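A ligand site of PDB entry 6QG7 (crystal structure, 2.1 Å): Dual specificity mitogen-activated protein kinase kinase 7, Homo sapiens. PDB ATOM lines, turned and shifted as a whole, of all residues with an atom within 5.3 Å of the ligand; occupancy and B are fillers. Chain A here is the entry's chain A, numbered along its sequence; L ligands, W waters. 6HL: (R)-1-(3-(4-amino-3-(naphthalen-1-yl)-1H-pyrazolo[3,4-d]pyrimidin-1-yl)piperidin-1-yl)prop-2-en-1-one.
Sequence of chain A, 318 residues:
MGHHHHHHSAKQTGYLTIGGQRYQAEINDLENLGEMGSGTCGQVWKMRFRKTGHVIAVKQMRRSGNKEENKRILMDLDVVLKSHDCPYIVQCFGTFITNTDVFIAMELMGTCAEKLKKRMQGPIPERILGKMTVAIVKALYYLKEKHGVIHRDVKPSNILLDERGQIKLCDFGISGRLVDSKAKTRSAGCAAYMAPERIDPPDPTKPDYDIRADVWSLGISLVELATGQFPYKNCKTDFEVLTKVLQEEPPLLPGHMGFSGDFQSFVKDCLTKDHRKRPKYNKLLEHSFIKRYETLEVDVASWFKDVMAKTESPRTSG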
ATOM      1  N   MET A  36     -12.203  -5.418   2.812  1.00  0.00           N
ATOM      2  CA  MET A  36     -11.078  -4.527   3.088  1.00  0.00           C
ATOM      3  C   MET A  36     -11.364  -3.749   4.361  1.00  0.00           C
ATOM      4  O   MET A  36     -12.386  -3.057   4.458  1.00  0.00           O
ATOM      5  CB  MET A  36     -10.847  -3.568   1.915  1.00  0.00           C
ATOM      6  CG  MET A  36     -10.228  -4.222   0.691  1.00  0.00           C
ATOM      7  SD  MET A  36      -9.472  -3.022  -0.412  1.00  0.00           S
ATOM      8  CE  MET A  36     -10.857  -1.917  -0.691  1.00  0.00           C
ATOM      9  N   GLY A  37     -10.470  -3.864   5.336  1.00  0.00           N
ATOM     10  CA  GLY A  37     -10.618  -3.148   6.589  1.00  0.00           C
ATOM     11  C   GLY A  37     -11.638  -3.766   7.522  1.00  0.00           C
ATOM     12  O   GLY A  37     -12.678  -4.269   7.078  1.00  0.00           O
ATOM     13  N   SER A  38     -11.346  -3.744   8.820  1.00  0.00           N
ATOM     14  CA  SER A  38     -12.261  -4.310   9.798  1.00  0.00           C
ATOM     15  C   SER A  38     -13.380  -3.339  10.168  1.00  0.00           C
ATOM     16  O   SER A  38     -14.541  -3.744  10.275  1.00  0.00           O
ATOM     17  CB  SER A  38     -11.491  -4.761  11.036  1.00  0.00           C
ATOM     18  OG  SER A  38     -10.222  -5.282  10.693  1.00  0.00           O
ATOM     19  N   GLY A  39     -13.052  -2.065  10.375  1.00  0.00           N
ATOM     20  CA  GLY A  39     -14.044  -1.084  10.775  1.00  0.00           C
ATOM     21  C   GLY A  39     -14.357  -0.096   9.675  1.00  0.00           C
ATOM     22  O   GLY A  39     -13.464   0.578   9.169  1.00  0.00           O
ATOM     23  N   THR A  40     -15.636   0.006   9.303  1.00  0.00           N
ATOM     24  CA  THR A  40     -16.001   0.760   8.118  1.00  0.00           C
ATOM     25  C   THR A  40     -17.149   1.713   8.461  1.00  0.00           C
ATOM     26  O   THR A  40     -17.582   1.829   9.610  1.00  0.00           O
ATOM     27  CB  THR A  40     -16.400  -0.192   6.981  1.00  0.00           C
ATOM     28  OG1 THR A  40     -17.443  -1.071   7.403  1.00  0.00           O
ATOM     29  CG2 THR A  40     -15.207  -1.001   6.495  1.00  0.00           C
ATOM     30  N   VAL A  44     -16.831  -2.528   2.497  1.00  0.00           N
ATOM     31  CA  VAL A  44     -15.989  -2.204   1.354  1.00  0.00           C
ATOM     32  C   VAL A  44     -15.311  -3.485   0.897  1.00  0.00           C
ATOM     33  O   VAL A  44     -14.526  -4.077   1.647  1.00  0.00           O
ATOM     34  CB  VAL A  44     -14.958  -1.113   1.697  1.00  0.00           C
ATOM     35  CG1 VAL A  44     -14.159  -0.742   0.458  1.00  0.00           C
ATOM     36  CG2 VAL A  44     -15.649   0.105   2.282  1.00  0.00           C
ATOM     37  N   ALA A  57     -12.470  -1.120  -5.664  1.00  0.00           N
ATOM     38  CA  ALA A  57     -13.068  -1.153  -4.340  1.00  0.00           C
ATOM     39  C   ALA A  57     -14.565  -0.872  -4.468  1.00  0.00           C
ATOM     40  O   ALA A  57     -14.964   0.185  -4.979  1.00  0.00           O
ATOM     41  CB  ALA A  57     -12.408  -0.129  -3.420  1.00  0.00           C
ATOM     42  N   LYS A  59     -18.139  -0.624  -2.434  1.00  0.00           N
ATOM     43  CA  LYS A  59     -18.857  -0.509  -1.174  1.00  0.00           C
ATOM     44  C   LYS A  59     -20.288  -0.999  -1.369  1.00  0.00           C
ATOM     45  O   LYS A  59     -20.984  -0.563  -2.282  1.00  0.00           O
ATOM     46  CB  LYS A  59     -18.850   0.932  -0.675  1.00  0.00           C
ATOM     47  CG  LYS A  59     -19.723   1.164   0.557  1.00  0.00           C
ATOM     48  CD  LYS A  59     -19.482   2.536   1.167  1.00  0.00           C
ATOM     49  CE  LYS A  59     -18.437   2.473   2.258  1.00  0.00           C
ATOM     50  NZ  LYS A  59     -18.212   3.803   2.896  1.00  0.00           N
ATOM     51  N   ASP A  76     -21.813  10.948   0.641  1.00  0.00           N
ATOM     52  CA  ASP A  76     -20.465  10.840   0.115  1.00  0.00           C
ATOM     53  C   ASP A  76     -20.490  10.531  -1.378  1.00  0.00           C
ATOM     54  O   ASP A  76     -19.730  11.135  -2.157  1.00  0.00           O
ATOM     55  CB  ASP A  76     -19.686   9.760   0.865  1.00  0.00           C
ATOM     56  CG  ASP A  76     -18.436   9.320   0.120  1.00  0.00           C
ATOM     57  OD1 ASP A  76     -17.431  10.069   0.148  1.00  0.00           O
ATOM     58  OD2 ASP A  76     -18.458   8.232  -0.494  1.00  0.00           O
ATOM     59  N   VAL A  90     -10.830  10.846  -4.430  1.00  0.00           N
ATOM     60  CA  VAL A  90     -11.017   9.462  -4.889  1.00  0.00           C
ATOM     61  C   VAL A  90     -12.201   9.402  -5.838  1.00  0.00           C
ATOM     62  O   VAL A  90     -13.302   9.868  -5.521  1.00  0.00           O
ATOM     63  CB  VAL A  90     -11.207   8.524  -3.680  1.00  0.00           C
ATOM     64  CG1 VAL A  90     -11.132   7.074  -4.130  1.00  0.00           C
ATOM     65  CG2 VAL A  90     -10.162   8.813  -2.614  1.00  0.00           C
ATOM     66  N   ILE A 104     -21.243   0.581  -4.867  1.00  0.00           N
ATOM     67  CA  ILE A 104     -20.561   1.797  -5.279  1.00  0.00           C
ATOM     68  C   ILE A 104     -19.114   1.425  -5.578  1.00  0.00           C
ATOM     69  O   ILE A 104     -18.323   1.212  -4.648  1.00  0.00           O
ATOM     70  CB  ILE A 104     -20.653   2.906  -4.216  1.00  0.00           C
ATOM     71  CG1 ILE A 104     -22.118   3.291  -3.983  1.00  0.00           C
ATOM     72  CG2 ILE A 104     -19.837   4.113  -4.636  1.00  0.00           C
ATOM     73  CD1 ILE A 104     -22.356   4.031  -2.700  1.00  0.00           C
ATOM     74  N   MET A 106     -15.400   2.258  -6.662  1.00  0.00           N
ATOM     75  CA  MET A 106     -14.539   3.435  -6.551  1.00  0.00           C
ATOM     76  C   MET A 106     -13.092   3.035  -6.803  1.00  0.00           C
ATOM     77  O   MET A 106     -12.754   1.847  -6.925  1.00  0.00           O
ATOM     78  CB  MET A 106     -14.668   4.094  -5.176  1.00  0.00           C
ATOM     79  CG  MET A 106     -16.073   4.584  -4.844  1.00  0.00           C
ATOM     80  SD  MET A 106     -16.316   6.334  -5.207  1.00  0.00           S
ATOM     81  CE  MET A 106     -14.779   7.018  -4.591  1.00  0.00           C
ATOM     82  N   GLU A 107     -12.237   4.044  -6.903  1.00  0.00           N
ATOM     83  CA  GLU A 107     -10.811   3.831  -7.112  1.00  0.00           C
ATOM     84  C   GLU A 107     -10.227   3.016  -5.959  1.00  0.00           C
ATOM     85  O   GLU A 107     -10.375   3.370  -4.789  1.00  0.00           O
ATOM     86  CB  GLU A 107     -10.102   5.189  -7.208  1.00  0.00           C
ATOM     87  CG  GLU A 107      -8.837   5.179  -8.039  1.00  0.00           C
ATOM     88  CD  GLU A 107      -8.248   6.571  -8.179  1.00  0.00           C
ATOM     89  OE1 GLU A 107      -7.096   6.693  -8.646  1.00  0.00           O
ATOM     90  OE2 GLU A 107      -8.940   7.548  -7.821  1.00  0.00           O
ATOM     91  N   LEU A 108      -9.565   1.912  -6.302  1.00  0.00           N
ATOM     92  CA  LEU A 108      -8.938   1.063  -5.294  1.00  0.00           C
ATOM     93  C   LEU A 108      -7.644   1.713  -4.849  1.00  0.00           C
ATOM     94  O   LEU A 108      -6.635   1.676  -5.551  1.00  0.00           O
ATOM     95  CB  LEU A 108      -8.685  -0.339  -5.847  1.00  0.00           C
ATOM     96  CG  LEU A 108      -7.887  -1.239  -4.908  1.00  0.00           C
ATOM     97  CD1 LEU A 108      -8.765  -1.788  -3.789  1.00  0.00           C
ATOM     98  CD2 LEU A 108      -7.206  -2.367  -5.663  1.00  0.00           C
ATOM     99  N   MET A 109      -7.666   2.318  -3.664  1.00  0.00           N
ATOM    100  CA  MET A 109      -6.480   2.910  -3.083  1.00  0.00           C
ATOM    101  C   MET A 109      -5.727   1.853  -2.269  1.00  0.00           C
ATOM    102  O   MET A 109      -6.184   0.723  -2.103  1.00  0.00           O
ATOM    103  CB  MET A 109      -6.844   4.125  -2.230  1.00  0.00           C
ATOM    104  CG  MET A 109      -7.574   5.220  -2.980  1.00  0.00           C
ATOM    105  SD  MET A 109      -6.553   5.982  -4.255  1.00  0.00           S
ATOM    106  CE  MET A 109      -5.358   6.857  -3.250  1.00  0.00           C
ATOM    107  N   GLY A 110      -4.563   2.229  -1.747  1.00  0.00           N
ATOM    108  CA  GLY A 110      -3.786   1.333  -0.917  1.00  0.00           C
ATOM    109  C   GLY A 110      -4.276   1.307   0.515  1.00  0.00           C
ATOM    110  O   GLY A 110      -4.901   0.338   0.951  1.00  0.00           O
ATOM    111  N   THR A 111      -4.001   2.379   1.256  1.00  0.00           N
ATOM    112  CA  THR A 111      -4.434   2.482   2.646  1.00  0.00           C
ATOM    113  C   THR A 111      -4.516   3.958   3.008  1.00  0.00           C
ATOM    114  O   THR A 111      -4.161   4.834   2.227  1.00  0.00           O
ATOM    115  CB  THR A 111      -3.472   1.741   3.582  1.00  0.00           C
ATOM    116  OG1 THR A 111      -4.079   1.595   4.875  1.00  0.00           O
ATOM    117  CG2 THR A 111      -2.163   2.503   3.728  1.00  0.00           C
ATOM    118  N   CYS A 112      -4.998   4.216   4.220  1.00  0.00           N
ATOM    119  CA  CYS A 112      -5.133   5.575   4.700  1.00  0.00           C
ATOM    120  C   CYS A 112      -3.843   6.026   5.402  1.00  0.00           C
ATOM    121  O   CYS A 112      -2.909   5.246   5.598  1.00  0.00           O
ATOM    122  CB  CYS A 112      -6.333   5.703   5.632  1.00  0.00           C
ATOM    123  SG  CYS A 112      -6.165   4.831   7.198  1.00  0.00           S
ATOM    124  N   ALA A 113      -3.809   7.304   5.766  1.00  0.00           N
ATOM    125  CA  ALA A 113      -2.649   7.854   6.461  1.00  0.00           C
ATOM    126  C   ALA A 113      -2.572   7.359   7.895  1.00  0.00           C
ATOM    127  O   ALA A 113      -1.480   7.275   8.471  1.00  0.00           O
ATOM    128  CB  ALA A 113      -2.672   9.375   6.413  1.00  0.00           C
ATOM    129  N   GLU A 114      -3.714   7.017   8.495  1.00  0.00           N
ATOM    130  CA  GLU A 114      -3.708   6.486   9.857  1.00  0.00           C
ATOM    131  C   GLU A 114      -3.039   5.119   9.903  1.00  0.00           C
ATOM    132  O   GLU A 114      -2.144   4.880  10.725  1.00  0.00           O
ATOM    133  CB  GLU A 114      -5.129   6.405  10.407  1.00  0.00           C
ATOM    134  CG  GLU A 114      -5.237   5.632  11.710  1.00  0.00           C
ATOM    135  CD  GLU A 114      -6.623   5.690  12.321  1.00  0.00           C
ATOM    136  OE1 GLU A 114      -7.613   5.533  11.572  1.00  0.00           O
ATOM    137  OE2 GLU A 114      -6.727   5.906  13.546  1.00  0.00           O
ATOM    138  N   LYS A 115      -3.461   4.203   9.033  1.00  0.00           N
ATOM    139  CA  LYS A 115      -2.826   2.888   8.983  1.00  0.00           C
ATOM    140  C   LYS A 115      -1.367   2.979   8.561  1.00  0.00           C
ATOM    141  O   LYS A 115      -0.544   2.149   8.968  1.00  0.00           O
ATOM    142  CB  LYS A 115      -3.586   1.965   8.027  1.00  0.00           C
ATOM    143  CG  LYS A 115      -5.012   1.661   8.460  1.00  0.00           C
ATOM    144  CD  LYS A 115      -5.048   0.887   9.774  1.00  0.00           C
ATOM    145  CE  LYS A 115      -6.471   0.555  10.191  1.00  0.00           C
ATOM    146  NZ  LYS A 115      -7.151  -0.303   9.172  1.00  0.00           N
ATOM    147  N   PRO A 156      -6.392  11.933   9.416  1.00  0.00           N
ATOM    148  CA  PRO A 156      -5.509  10.991   8.705  1.00  0.00           C
ATOM    149  C   PRO A 156      -6.220   9.786   8.123  1.00  0.00           C
ATOM    150  O   PRO A 156      -5.820   9.308   7.048  1.00  0.00           O
ATOM    151  CB  PRO A 156      -4.502  10.574   9.799  1.00  0.00           C
ATOM    152  CG  PRO A 156      -4.459  11.749  10.710  1.00  0.00           C
ATOM    153  CD  PRO A 156      -5.847  12.306  10.735  1.00  0.00           C
ATOM    154  N   SER A 157      -7.265   9.275   8.778  1.00  0.00           N
ATOM    155  CA  SER A 157      -7.977   8.126   8.239  1.00  0.00           C
ATOM    156  C   SER A 157      -8.717   8.454   6.957  1.00  0.00           C
ATOM    157  O   SER A 157      -9.116   7.536   6.229  1.00  0.00           O
ATOM    158  CB  SER A 157      -8.964   7.581   9.284  1.00  0.00           C
ATOM    159  OG  SER A 157     -10.165   8.330   9.283  1.00  0.00           O
ATOM    160  N   LEU A 160      -6.117   9.021   1.648  1.00  0.00           N
ATOM    161  CA  LEU A 160      -5.810   7.730   1.028  1.00  0.00           C
ATOM    162  C   LEU A 160      -4.601   7.851   0.111  1.00  0.00           C
ATOM    163  O   LEU A 160      -4.450   8.827  -0.624  1.00  0.00           O
ATOM    164  CB  LEU A 160      -7.014   7.211   0.245  1.00  0.00           C
ATOM    165  CG  LEU A 160      -7.966   6.235   0.950  1.00  0.00           C
ATOM    166  CD1 LEU A 160      -8.228   6.659   2.388  1.00  0.00           C
ATOM    167  CD2 LEU A 160      -9.269   6.108   0.179  1.00  0.00           C
ATOM    168  N   CYS A 170     -11.173  11.300   0.738  1.00  0.00           N
ATOM    169  CA  CYS A 170     -12.019  10.130   0.529  1.00  0.00           C
ATOM    170  C   CYS A 170     -13.466  10.220   1.026  1.00  0.00           C
ATOM    171  O   CYS A 170     -14.391   9.910   0.270  1.00  0.00           O
ATOM    172  CB  CYS A 170     -11.364   8.908   1.158  1.00  0.00           C
ATOM    173  SG  CYS A 170     -11.620   8.698   2.932  1.00  0.00           S
ATOM    174  N   ASP A 171     -13.686  10.585   2.292  1.00  0.00           N
ATOM    175  CA  ASP A 171     -14.975  10.386   2.940  1.00  0.00           C
ATOM    176  C   ASP A 171     -15.704  11.715   3.115  1.00  0.00           C
ATOM    177  O   ASP A 171     -15.298  12.546   3.930  1.00  0.00           O
ATOM    178  CB  ASP A 171     -14.797   9.699   4.297  1.00  0.00           C
ATOM    179  CG  ASP A 171     -16.083   9.034   4.788  1.00  0.00           C
ATOM    180  OD1 ASP A 171     -17.173   9.371   4.272  1.00  0.00           O
ATOM    181  OD2 ASP A 171     -15.994   8.174   5.690  1.00  0.00           O
HETATM  182  C4  6HL L   1     -10.673   2.125   1.073  1.00  0.00           C
HETATM  183  C5  6HL L   1     -11.463   2.517   0.072  1.00  0.00           C
HETATM  184  C6  6HL L   1     -10.990   2.320  -1.189  1.00  0.00           C
HETATM  185  N1  6HL L   1      -9.788   1.779  -1.443  1.00  0.00           N
HETATM  186  N3  6HL L   1      -9.464   1.589   0.882  1.00  0.00           N
HETATM  187  CBC 6HL L   1      -7.827   4.444   7.172  1.00  0.00           C
HETATM  188  CBB 6HL L   1      -8.815   3.997   6.101  1.00  0.00           C
HETATM  189  CAZ 6HL L   1      -9.141   2.528   6.352  1.00  0.00           C
HETATM  190  OBA 6HL L   1      -8.491   1.914   7.200  1.00  0.00           O
HETATM  191  NAW 6HL L   1     -10.258   2.029   5.814  1.00  0.00           N
HETATM  192  CAX 6HL L   1     -11.101   2.587   4.733  1.00  0.00           C
HETATM  193  CAV 6HL L   1     -10.531   0.610   6.071  1.00  0.00           C
HETATM  194  CAU 6HL L   1      -9.957  -0.063   4.865  1.00  0.00           C
HETATM  195  CAT 6HL L   1     -10.686   0.474   3.612  1.00  0.00           C
HETATM  196  CAY 6HL L   1     -10.538   1.994   3.452  1.00  0.00           C
HETATM  197  NAM 6HL L   1     -11.256   2.420   2.226  1.00  0.00           N
HETATM  198  NAN 6HL L   1     -12.301   2.907   2.024  1.00  0.00           N
HETATM  199  C2  6HL L   1      -8.968   1.387  -0.398  1.00  0.00           C
HETATM  200  NBD 6HL L   1     -11.686   2.675  -2.245  1.00  0.00           N
HETATM  201  CAO 6HL L   1     -12.586   2.952   0.717  1.00  0.00           C
HETATM  202  CAC 6HL L   1     -13.702   3.534   0.205  1.00  0.00           C
HETATM  203  CAD 6HL L   1     -14.459   4.570   0.804  1.00  0.00           C
HETATM  204  CAG 6HL L   1     -14.188   5.060   2.085  1.00  0.00           C
HETATM  205  CAH 6HL L   1     -14.972   6.039   2.670  1.00  0.00           C
HETATM  206  CAI 6HL L   1     -16.054   6.578   1.992  1.00  0.00           C
HETATM  207  CAJ 6HL L   1     -16.339   6.113   0.720  1.00  0.00           C
HETATM  208  CAE 6HL L   1     -15.558   5.121   0.133  1.00  0.00           C
HETATM  209  CAF 6HL L   1     -15.917   4.723  -1.137  1.00  0.00           C
HETATM  210  CAA 6HL L   1     -15.173   3.745  -1.753  1.00  0.00           C
HETATM  211  CAB 6HL L   1     -14.075   3.233  -1.095  1.00  0.00           C
HETATM  212  O   HOH W   1     -13.392   6.549   5.239  1.00  0.00           O
HETATM  213  O   HOH W   2     -10.898   6.150   4.948  1.00  0.00           O
HETATM  214  O   HOH W   3     -15.635   8.577  -1.331  1.00  0.00           O
HETATM  215  O   HOH W   4     -15.342   3.185   4.210  1.00  0.00           O
HETATM  216  O   HOH W   5      -7.360   0.043   2.774  1.00  0.00           O
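Residues that only touch the ligand: Ala 57, Asp 76, Met 106, Ser 157, Gly 37, Lys 59, Asp 171 and Met 36.
Hydrophobic or aromatic side chains within 4 Å of the ligand: Met 36, Ala 57, Met 106 and Met 109.
12 residues have an atom within 4 Å of the ligand: Met 36, Gly 37, Ala 57, Lys 59, Asp 76, Met 106, Glu 107, Met 109, Cys 112, Lys 115, Ser 157 and Asp 171.
The nearest printed residue that does not touch the ligand is Leu 108 (4.01 Å).
The backbone carbonyl oxygen (O) of Lys 59 lies within hydrogen-bond range of the backbone NH (N) of Ile 104 (2.8 Å).
SG of Cys 112 sits close to N of Glu 114 (3.5 Å).
The backbone NH of Met 106 is in hydrogen-bond range of the backbone carbonyl oxygen of Ala 57 (2.7 Å).
The backbone NH (N) of Met 36 sits at hydrogen-bond distance from the backbone carbonyl oxygen (O) of Val 44 (2.9 Å).
The side-chain sulfur (SG) of Cys 112 sits at hydrogen-bond distance from the backbone NH (N) of Lys 115, at 3.3 Å.
Water W1 bridges OD2 of Asp 171 (3.1 Å) and SG of Cys 170 (3.6 Å).
Water W2 bridges the backbone carbonyl oxygen (O) of Ser 157 and the side-chain sulfur (SG) of Cys 170.
Water W5 lies within hydrogen-bond range of the backbone carbonyl oxygen of Gly 110 (3.1 Å) and a nitrogen (N3) of the ligand (3.2 Å).
Water W3 bridges the backbone carbonyl oxygen of Cys 170 and the side-chain carboxylate of Asp 76.
The side-chain sulfur (SG) of Cys 112 is bonded to a carbon (CBC) of the ligand, 1.7 Å away.
The backbone NH (N) of Met 109 is in hydrogen-bond range of a nitrogen (N1) of the ligand, at 3.1 Å.
The side-chain amino group (NZ) of Lys 115 sits at hydrogen-bond distance from an oxygen (OBA) of the ligand, 3.3 Å away.
The backbone carbonyl oxygen (O) of Glu 107 is in hydrogen-bond range of a nitrogen (NBD) of the ligand, at 2.9 Å.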
